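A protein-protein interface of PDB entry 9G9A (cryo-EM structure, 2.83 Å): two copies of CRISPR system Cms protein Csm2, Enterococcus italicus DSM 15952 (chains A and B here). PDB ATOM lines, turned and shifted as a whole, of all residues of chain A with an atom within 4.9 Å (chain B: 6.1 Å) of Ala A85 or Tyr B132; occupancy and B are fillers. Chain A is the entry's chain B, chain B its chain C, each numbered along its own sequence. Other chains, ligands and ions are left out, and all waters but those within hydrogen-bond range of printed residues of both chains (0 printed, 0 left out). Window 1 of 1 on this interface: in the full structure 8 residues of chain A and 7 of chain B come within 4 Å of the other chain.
The guanidinium group of Arg B18 is in hydrogen-bond range of the side-chain hydroxyl of Tyr B136 (3.1 Å).
Of the printed residues of chain B, Val A82 touches Ala B128 (3.8 Å). Ala A85 touches just these residues of chain B: Tyr B132 (3.5 Å) and Phe B135 (3.7 Å). Printed residues of chain B within 4 Å of Tyr A86: Ala B131. Of the printed residues of chain A, Glu B127 touches Lys A83. Leu B129 touches none of the printed residues of chain A. Printed residues of chain A within 4 Å of Ala B131: Tyr A86 (3.7 Å). Of chain A, only Lys A81 (3.7 Å) and Ala A85 (3.5 Å) come within 4 Å of Tyr B132. Of the printed residues of chain A, Phe B135 touches Ala A85 and Ser A88. Tyr B136 touches none of the printed residues of chain A. The nearest printed residue of chain B that does not touch Lys A81 is Asn B15 (6.4 Å).
NZ of Lys A81 touches NH1 of Arg B18, 3.9 Å away. NZ of Lys A81 touches OH of Tyr B132, at 3.7 Å. Val A82 touches Ala B128 (CG1 to CB, 3.8 Å). Ala A85 touches Tyr B132 (CB to CE1, 3.5 Å). O of Ala A85 touches CD2 of Phe B135, 3.7 Å away. CB of Ala B131 touches CB of Tyr A86, at 3.7 Å. Phe B135 touches Ser A88.
Of the 9 printed residues of chain A, 6 touch a printed residue of chain B. Hydrophobic or aromatic side chains of chain A within 4 Å of the printed part of chain B: Val A82, Ala A85 and Tyr A86.
No position is printed for both chains. Of the 8 pairs that touch across the chains among the printed residues, none has its exchanged pair printed and touching as well.
NZ of Lys A83 lies within salt-bridge range of OE2 of Glu B127 (2.8 Å).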
ATOM      1  N   LYS A  81      28.747  -1.915 -20.470  1.00  0.00           N
ATOM      2  CA  LYS A  81      28.833  -1.674 -21.911  1.00  0.00           C
ATOM      3  C   LYS A  81      28.419  -2.912 -22.700  1.00  0.00           C
ATOM      4  O   LYS A  81      27.743  -2.806 -23.735  1.00  0.00           O
ATOM      5  CB  LYS A  81      30.247  -1.240 -22.298  1.00  0.00           C
ATOM      6  CG  LYS A  81      30.364  -0.814 -23.752  1.00  0.00           C
ATOM      7  CD  LYS A  81      31.804  -0.558 -24.156  1.00  0.00           C
ATOM      8  CE  LYS A  81      31.884  -0.062 -25.592  1.00  0.00           C
ATOM      9  NZ  LYS A  81      31.201  -0.983 -26.542  1.00  0.00           N
ATOM     10  N   VAL A  82      28.819  -4.095 -22.228  1.00  0.00           N
ATOM     11  CA  VAL A  82      28.405  -5.334 -22.883  1.00  0.00           C
ATOM     12  C   VAL A  82      26.886  -5.464 -22.862  1.00  0.00           C
ATOM     13  O   VAL A  82      26.262  -5.834 -23.866  1.00  0.00           O
ATOM     14  CB  VAL A  82      29.089  -6.546 -22.222  1.00  0.00           C
ATOM     15  CG1 VAL A  82      28.524  -7.846 -22.773  1.00  0.00           C
ATOM     16  CG2 VAL A  82      30.593  -6.488 -22.435  1.00  0.00           C
ATOM     17  N   LYS A  83      26.265  -5.154 -21.722  1.00  0.00           N
ATOM     18  CA  LYS A  83      24.812  -5.212 -21.622  1.00  0.00           C
ATOM     19  C   LYS A  83      24.149  -4.133 -22.470  1.00  0.00           C
ATOM     20  O   LYS A  83      23.055  -4.353 -23.000  1.00  0.00           O
ATOM     21  CB  LYS A  83      24.380  -5.086 -20.160  1.00  0.00           C
ATOM     22  CG  LYS A  83      23.021  -5.700 -19.860  1.00  0.00           C
ATOM     23  CD  LYS A  83      23.026  -7.198 -20.126  1.00  0.00           C
ATOM     24  CE  LYS A  83      24.053  -7.912 -19.261  1.00  0.00           C
ATOM     25  NZ  LYS A  83      24.146  -9.364 -19.579  1.00  0.00           N
ATOM     26  N   PHE A  84      24.788  -2.968 -22.603  1.00  0.00           N
ATOM     27  CA  PHE A  84      24.301  -1.948 -23.526  1.00  0.00           C
ATOM     28  C   PHE A  84      24.231  -2.498 -24.943  1.00  0.00           C
ATOM     29  O   PHE A  84      23.221  -2.344 -25.635  1.00  0.00           O
ATOM     30  CB  PHE A  84      25.212  -0.718 -23.490  1.00  0.00           C
ATOM     31  CG  PHE A  84      24.938   0.219 -22.350  1.00  0.00           C
ATOM     32  CD1 PHE A  84      23.779   0.113 -21.605  1.00  0.00           C
ATOM     33  CD2 PHE A  84      25.843   1.219 -22.035  1.00  0.00           C
ATOM     34  CE1 PHE A  84      23.532   0.983 -20.561  1.00  0.00           C
ATOM     35  CE2 PHE A  84      25.598   2.090 -20.994  1.00  0.00           C
ATOM     36  CZ  PHE A  84      24.442   1.971 -20.256  1.00  0.00           C
ATOM     37  N   ALA A  85      25.309  -3.147 -25.386  1.00  0.00           N
ATOM     38  CA  ALA A  85      25.324  -3.730 -26.725  1.00  0.00           C
ATOM     39  C   ALA A  85      24.275  -4.827 -26.862  1.00  0.00           C
ATOM     40  O   ALA A  85      23.591  -4.922 -27.889  1.00  0.00           O
ATOM     41  CB  ALA A  85      26.715  -4.273 -27.045  1.00  0.00           C
ATOM     42  N   TYR A  86      24.135  -5.666 -25.834  1.00  0.00           N
ATOM     43  CA  TYR A  86      23.166  -6.758 -25.883  1.00  0.00           C
ATOM     44  C   TYR A  86      21.740  -6.230 -25.994  1.00  0.00           C
ATOM     45  O   TYR A  86      20.945  -6.718 -26.806  1.00  0.00           O
ATOM     46  CB  TYR A  86      23.325  -7.642 -24.646  1.00  0.00           C
ATOM     47  CG  TYR A  86      22.276  -8.723 -24.511  1.00  0.00           C
ATOM     48  CD1 TYR A  86      22.116  -9.690 -25.494  1.00  0.00           C
ATOM     49  CD2 TYR A  86      21.459  -8.786 -23.391  1.00  0.00           C
ATOM     50  CE1 TYR A  86      21.163 -10.683 -25.371  1.00  0.00           C
ATOM     51  CE2 TYR A  86      20.506  -9.775 -23.258  1.00  0.00           C
ATOM     52  CZ  TYR A  86      20.361 -10.720 -24.251  1.00  0.00           C
ATOM     53  OH  TYR A  86      19.410 -11.707 -24.125  1.00  0.00           O
ATOM     54  N   GLU A  87      21.399  -5.220 -25.188  1.00  0.00           N
ATOM     55  CA  GLU A  87      20.059  -4.647 -25.241  1.00  0.00           C
ATOM     56  C   GLU A  87      19.825  -3.875 -26.532  1.00  0.00           C
ATOM     57  O   GLU A  87      18.707  -3.879 -27.060  1.00  0.00           O
ATOM     58  CB  GLU A  87      19.823  -3.748 -24.028  1.00  0.00           C
ATOM     59  CG  GLU A  87      19.790  -4.492 -22.702  1.00  0.00           C
ATOM     60  CD  GLU A  87      18.587  -5.407 -22.573  1.00  0.00           C
ATOM     61  OE1 GLU A  87      17.583  -5.180 -23.280  1.00  0.00           O
ATOM     62  OE2 GLU A  87      18.644  -6.357 -21.763  1.00  0.00           O
ATOM     63  N   SER A  88      20.857  -3.203 -27.051  1.00  0.00           N
ATOM     64  CA  SER A  88      20.735  -2.533 -28.340  1.00  0.00           C
ATOM     65  C   SER A  88      20.439  -3.533 -29.448  1.00  0.00           C
ATOM     66  O   SER A  88      19.604  -3.276 -30.321  1.00  0.00           O
ATOM     67  CB  SER A  88      22.015  -1.753 -28.639  1.00  0.00           C
ATOM     68  OG  SER A  88      22.066  -1.337 -29.990  1.00  0.00           O
ATOM     69  N   GLY A  89      21.116  -4.681 -29.428  1.00  0.00           N
ATOM     70  CA  GLY A  89      20.811  -5.719 -30.397  1.00  0.00           C
ATOM     71  C   GLY A  89      19.427  -6.310 -30.204  1.00  0.00           C
ATOM     72  O   GLY A  89      18.735  -6.624 -31.177  1.00  0.00           O
ATOM     73  N   ASN B  15      36.983  -4.125 -25.163  1.00  0.00           N
ATOM     74  CA  ASN B  15      36.827  -5.565 -25.004  1.00  0.00           C
ATOM     75  C   ASN B  15      37.295  -6.297 -26.259  1.00  0.00           C
ATOM     76  O   ASN B  15      37.029  -5.860 -27.378  1.00  0.00           O
ATOM     77  CB  ASN B  15      35.372  -5.917 -24.695  1.00  0.00           C
ATOM     78  CG  ASN B  15      35.205  -7.349 -24.227  1.00  0.00           C
ATOM     79  OD1 ASN B  15      36.141  -7.959 -23.714  1.00  0.00           O
ATOM     80  ND2 ASN B  15      34.006  -7.893 -24.402  1.00  0.00           N
ATOM     81  N   ALA B  17      36.265  -9.093 -27.355  1.00  0.00           N
ATOM     82  CA  ALA B  17      35.155  -9.762 -28.027  1.00  0.00           C
ATOM     83  C   ALA B  17      34.609  -8.933 -29.183  1.00  0.00           C
ATOM     84  O   ALA B  17      34.322  -9.462 -30.264  1.00  0.00           O
ATOM     85  CB  ALA B  17      34.048 -10.067 -27.015  1.00  0.00           C
ATOM     86  N   ARG B  18      34.459  -7.623 -28.971  1.00  0.00           N
ATOM     87  CA  ARG B  18      33.903  -6.764 -30.011  1.00  0.00           C
ATOM     88  C   ARG B  18      34.794  -6.739 -31.246  1.00  0.00           C
ATOM     89  O   ARG B  18      34.296  -6.803 -32.377  1.00  0.00           O
ATOM     90  CB  ARG B  18      33.700  -5.351 -29.468  1.00  0.00           C
ATOM     91  CG  ARG B  18      33.022  -4.401 -30.443  1.00  0.00           C
ATOM     92  CD  ARG B  18      32.887  -3.009 -29.847  1.00  0.00           C
ATOM     93  NE  ARG B  18      32.243  -2.076 -30.766  1.00  0.00           N
ATOM     94  CZ  ARG B  18      30.943  -1.822 -30.787  1.00  0.00           C
ATOM     95  NH1 ARG B  18      30.107  -2.422 -29.955  1.00  0.00           N
ATOM     96  NH2 ARG B  18      30.467  -0.944 -31.665  1.00  0.00           N
ATOM     97  N   LYS B  19      36.112  -6.655 -31.050  1.00  0.00           N
ATOM     98  CA  LYS B  19      37.026  -6.585 -32.186  1.00  0.00           C
ATOM     99  C   LYS B  19      36.963  -7.850 -33.032  1.00  0.00           C
ATOM    100  O   LYS B  19      36.851  -7.776 -34.261  1.00  0.00           O
ATOM    101  CB  LYS B  19      38.452  -6.337 -31.695  1.00  0.00           C
ATOM    102  CG  LYS B  19      39.511  -6.410 -32.788  1.00  0.00           C
ATOM    103  CD  LYS B  19      39.229  -5.420 -33.908  1.00  0.00           C
ATOM    104  CE  LYS B  19      39.297  -3.985 -33.414  1.00  0.00           C
ATOM    105  NZ  LYS B  19      38.966  -3.019 -34.497  1.00  0.00           N
ATOM    106  N   VAL B  21      34.561 -10.069 -33.123  1.00  0.00           N
ATOM    107  CA  VAL B  21      33.224 -10.208 -33.697  1.00  0.00           C
ATOM    108  C   VAL B  21      33.084  -9.342 -34.944  1.00  0.00           C
ATOM    109  O   VAL B  21      32.570  -9.790 -35.977  1.00  0.00           O
ATOM    110  CB  VAL B  21      32.148  -9.874 -32.649  1.00  0.00           C
ATOM    111  CG1 VAL B  21      30.831  -9.539 -33.327  1.00  0.00           C
ATOM    112  CG2 VAL B  21      31.961 -11.046 -31.699  1.00  0.00           C
ATOM    113  N   LEU B  38      28.868 -11.449 -40.603  1.00  0.00           N
ATOM    114  CA  LEU B  38      29.068 -12.533 -39.649  1.00  0.00           C
ATOM    115  C   LEU B  38      29.084 -13.882 -40.357  1.00  0.00           C
ATOM    116  O   LEU B  38      28.772 -13.974 -41.544  1.00  0.00           O
ATOM    117  CB  LEU B  38      27.977 -12.520 -38.571  1.00  0.00           C
ATOM    118  CG  LEU B  38      27.961 -11.382 -37.543  1.00  0.00           C
ATOM    119  CD1 LEU B  38      29.358 -11.121 -36.995  1.00  0.00           C
ATOM    120  CD2 LEU B  38      27.344 -10.106 -38.109  1.00  0.00           C
ATOM    121  N   GLU B 127      29.414 -14.555 -23.570  1.00  0.00           N
ATOM    122  CA  GLU B 127      28.185 -13.783 -23.688  1.00  0.00           C
ATOM    123  C   GLU B 127      28.425 -12.486 -24.447  1.00  0.00           C
ATOM    124  O   GLU B 127      27.571 -12.047 -25.220  1.00  0.00           O
ATOM    125  CB  GLU B 127      27.608 -13.490 -22.303  1.00  0.00           C
ATOM    126  CG  GLU B 127      26.264 -12.779 -22.334  1.00  0.00           C
ATOM    127  CD  GLU B 127      25.952 -12.064 -21.036  1.00  0.00           C
ATOM    128  OE1 GLU B 127      26.900 -11.764 -20.280  1.00  0.00           O
ATOM    129  OE2 GLU B 127      24.761 -11.802 -20.770  1.00  0.00           O
ATOM    130  N   ALA B 128      29.579 -11.852 -24.227  1.00  0.00           N
ATOM    131  CA  ALA B 128      29.923 -10.649 -24.975  1.00  0.00           C
ATOM    132  C   ALA B 128      30.086 -10.954 -26.457  1.00  0.00           C
ATOM    133  O   ALA B 128      29.652 -10.172 -27.307  1.00  0.00           O
ATOM    134  CB  ALA B 128      31.199 -10.026 -24.410  1.00  0.00           C
ATOM    135  N   LEU B 129      30.715 -12.086 -26.784  1.00  0.00           N
ATOM    136  CA  LEU B 129      30.810 -12.502 -28.181  1.00  0.00           C
ATOM    137  C   LEU B 129      29.429 -12.635 -28.808  1.00  0.00           C
ATOM    138  O   LEU B 129      29.169 -12.088 -29.887  1.00  0.00           O
ATOM    139  CB  LEU B 129      31.556 -13.831 -28.289  1.00  0.00           C
ATOM    140  CG  LEU B 129      33.055 -13.884 -28.010  1.00  0.00           C
ATOM    141  CD1 LEU B 129      33.507 -15.331 -27.988  1.00  0.00           C
ATOM    142  CD2 LEU B 129      33.816 -13.104 -29.066  1.00  0.00           C
ATOM    143  N   VAL B 130      28.530 -13.359 -28.137  1.00  0.00           N
ATOM    144  CA  VAL B 130      27.188 -13.573 -28.679  1.00  0.00           C
ATOM    145  C   VAL B 130      26.438 -12.251 -28.800  1.00  0.00           C
ATOM    146  O   VAL B 130      25.756 -11.992 -29.801  1.00  0.00           O
ATOM    147  CB  VAL B 130      26.419 -14.584 -27.811  1.00  0.00           C
ATOM    148  CG1 VAL B 130      25.024 -14.814 -28.369  1.00  0.00           C
ATOM    149  CG2 VAL B 130      27.185 -15.891 -27.727  1.00  0.00           C
ATOM    150  N   ALA B 131      26.547 -11.397 -27.780  1.00  0.00           N
ATOM    151  CA  ALA B 131      25.836 -10.124 -27.782  1.00  0.00           C
ATOM    152  C   ALA B 131      26.339  -9.209 -28.888  1.00  0.00           C
ATOM    153  O   ALA B 131      25.542  -8.544 -29.555  1.00  0.00           O
ATOM    154  CB  ALA B 131      25.974  -9.448 -26.419  1.00  0.00           C
ATOM    155  N   TYR B 132      27.656  -9.153 -29.096  1.00  0.00           N
ATOM    156  CA  TYR B 132      28.194  -8.331 -30.174  1.00  0.00           C
ATOM    157  C   TYR B 132      27.809  -8.890 -31.537  1.00  0.00           C
ATOM    158  O   TYR B 132      27.544  -8.128 -32.475  1.00  0.00           O
ATOM    159  CB  TYR B 132      29.713  -8.218 -30.041  1.00  0.00           C
ATOM    160  CG  TYR B 132      30.160  -7.255 -28.963  1.00  0.00           C
ATOM    161  CD1 TYR B 132      29.604  -5.987 -28.865  1.00  0.00           C
ATOM    162  CD2 TYR B 132      31.131  -7.616 -28.040  1.00  0.00           C
ATOM    163  CE1 TYR B 132      30.009  -5.104 -27.882  1.00  0.00           C
ATOM    164  CE2 TYR B 132      31.540  -6.742 -27.051  1.00  0.00           C
ATOM    165  CZ  TYR B 132      30.975  -5.486 -26.978  1.00  0.00           C
ATOM    166  OH  TYR B 132      31.379  -4.610 -25.997  1.00  0.00           O
ATOM    167  N   ALA B 133      27.770 -10.220 -31.669  1.00  0.00           N
ATOM    168  CA  ALA B 133      27.321 -10.814 -32.923  1.00  0.00           C
ATOM    169  C   ALA B 133      25.871 -10.450 -33.215  1.00  0.00           C
ATOM    170  O   ALA B 133      25.517 -10.140 -34.359  1.00  0.00           O
ATOM    171  CB  ALA B 133      27.499 -12.331 -32.878  1.00  0.00           C
ATOM    172  N   LYS B 134      25.016 -10.485 -32.190  1.00  0.00           N
ATOM    173  CA  LYS B 134      23.629 -10.064 -32.365  1.00  0.00           C
ATOM    174  C   LYS B 134      23.538  -8.573 -32.672  1.00  0.00           C
ATOM    175  O   LYS B 134      22.703  -8.144 -33.477  1.00  0.00           O
ATOM    176  CB  LYS B 134      22.817 -10.410 -31.116  1.00  0.00           C
ATOM    177  CG  LYS B 134      21.343 -10.039 -31.205  1.00  0.00           C
ATOM    178  CD  LYS B 134      20.571 -10.467 -29.960  1.00  0.00           C
ATOM    179  CE  LYS B 134      20.113 -11.921 -30.033  1.00  0.00           C
ATOM    180  NZ  LYS B 134      21.224 -12.906 -29.902  1.00  0.00           N
ATOM    181  N   PHE B 135      24.382  -7.767 -32.024  1.00  0.00           N
ATOM    182  CA  PHE B 135      24.365  -6.322 -32.229  1.00  0.00           C
ATOM    183  C   PHE B 135      24.741  -5.956 -33.658  1.00  0.00           C
ATOM    184  O   PHE B 135      24.117  -5.079 -34.268  1.00  0.00           O
ATOM    185  CB  PHE B 135      25.311  -5.655 -31.229  1.00  0.00           C
ATOM    186  CG  PHE B 135      25.548  -4.194 -31.488  1.00  0.00           C
ATOM    187  CD1 PHE B 135      26.675  -3.771 -32.174  1.00  0.00           C
ATOM    188  CD2 PHE B 135      24.652  -3.243 -31.032  1.00  0.00           C
ATOM    189  CE1 PHE B 135      26.896  -2.430 -32.410  1.00  0.00           C
ATOM    190  CE2 PHE B 135      24.870  -1.899 -31.265  1.00  0.00           C
ATOM    191  CZ  PHE B 135      25.993  -1.493 -31.954  1.00  0.00           C
ATOM    192  N   TYR B 136      25.760  -6.614 -34.211  1.00  0.00           N
ATOM    193  CA  TYR B 136      26.205  -6.268 -35.557  1.00  0.00           C
ATOM    194  C   TYR B 136      25.282  -6.852 -36.620  1.00  0.00           C
ATOM    195  O   TYR B 136      25.329  -6.440 -37.785  1.00  0.00           O
ATOM    196  CB  TYR B 136      27.646  -6.737 -35.771  1.00  0.00           C
ATOM    197  CG  TYR B 136      28.673  -5.800 -35.175  1.00  0.00           C
ATOM    198  CD1 TYR B 136      29.322  -6.109 -33.988  1.00  0.00           C
ATOM    199  CD2 TYR B 136      28.984  -4.597 -35.796  1.00  0.00           C
ATOM    200  CE1 TYR B 136      30.257  -5.251 -33.441  1.00  0.00           C
ATOM    201  CE2 TYR B 136      29.917  -3.734 -35.257  1.00  0.00           C
ATOM    202  CZ  TYR B 136      30.550  -4.066 -34.079  1.00  0.00           C
ATOM    203  OH  TYR B 136      31.480  -3.207 -33.540  1.00  0.00           O
ATOM    204  N   ARG B 137      24.436  -7.805 -36.243  1.00  0.00           N
ATOM    205  CA  ARG B 137      23.503  -8.402 -37.193  1.00  0.00           C
ATOM    206  C   ARG B 137      22.137  -7.731 -37.109  1.00  0.00           C
ATOM    207  O   ARG B 137      22.036  -6.534 -36.843  1.00  0.00           O
ATOM    208  CB  ARG B 137      23.361  -9.904 -36.945  1.00  0.00           C
ATOM    209  CG  ARG B 137      22.420 -10.260 -35.806  1.00  0.00           C
ATOM    210  CD  ARG B 137      22.330 -11.764 -35.590  1.00  0.00           C
ATOM    211  NE  ARG B 137      23.596 -12.337 -35.146  1.00  0.00           N
ATOM    212  CZ  ARG B 137      24.463 -12.947 -35.943  1.00  0.00           C
ATOM    213  NH1 ARG B 137      24.229 -13.092 -37.237  1.00  0.00           N
ATOM    214  NH2 ARG B 137      25.594 -13.421 -35.429  1.00  0.00           N
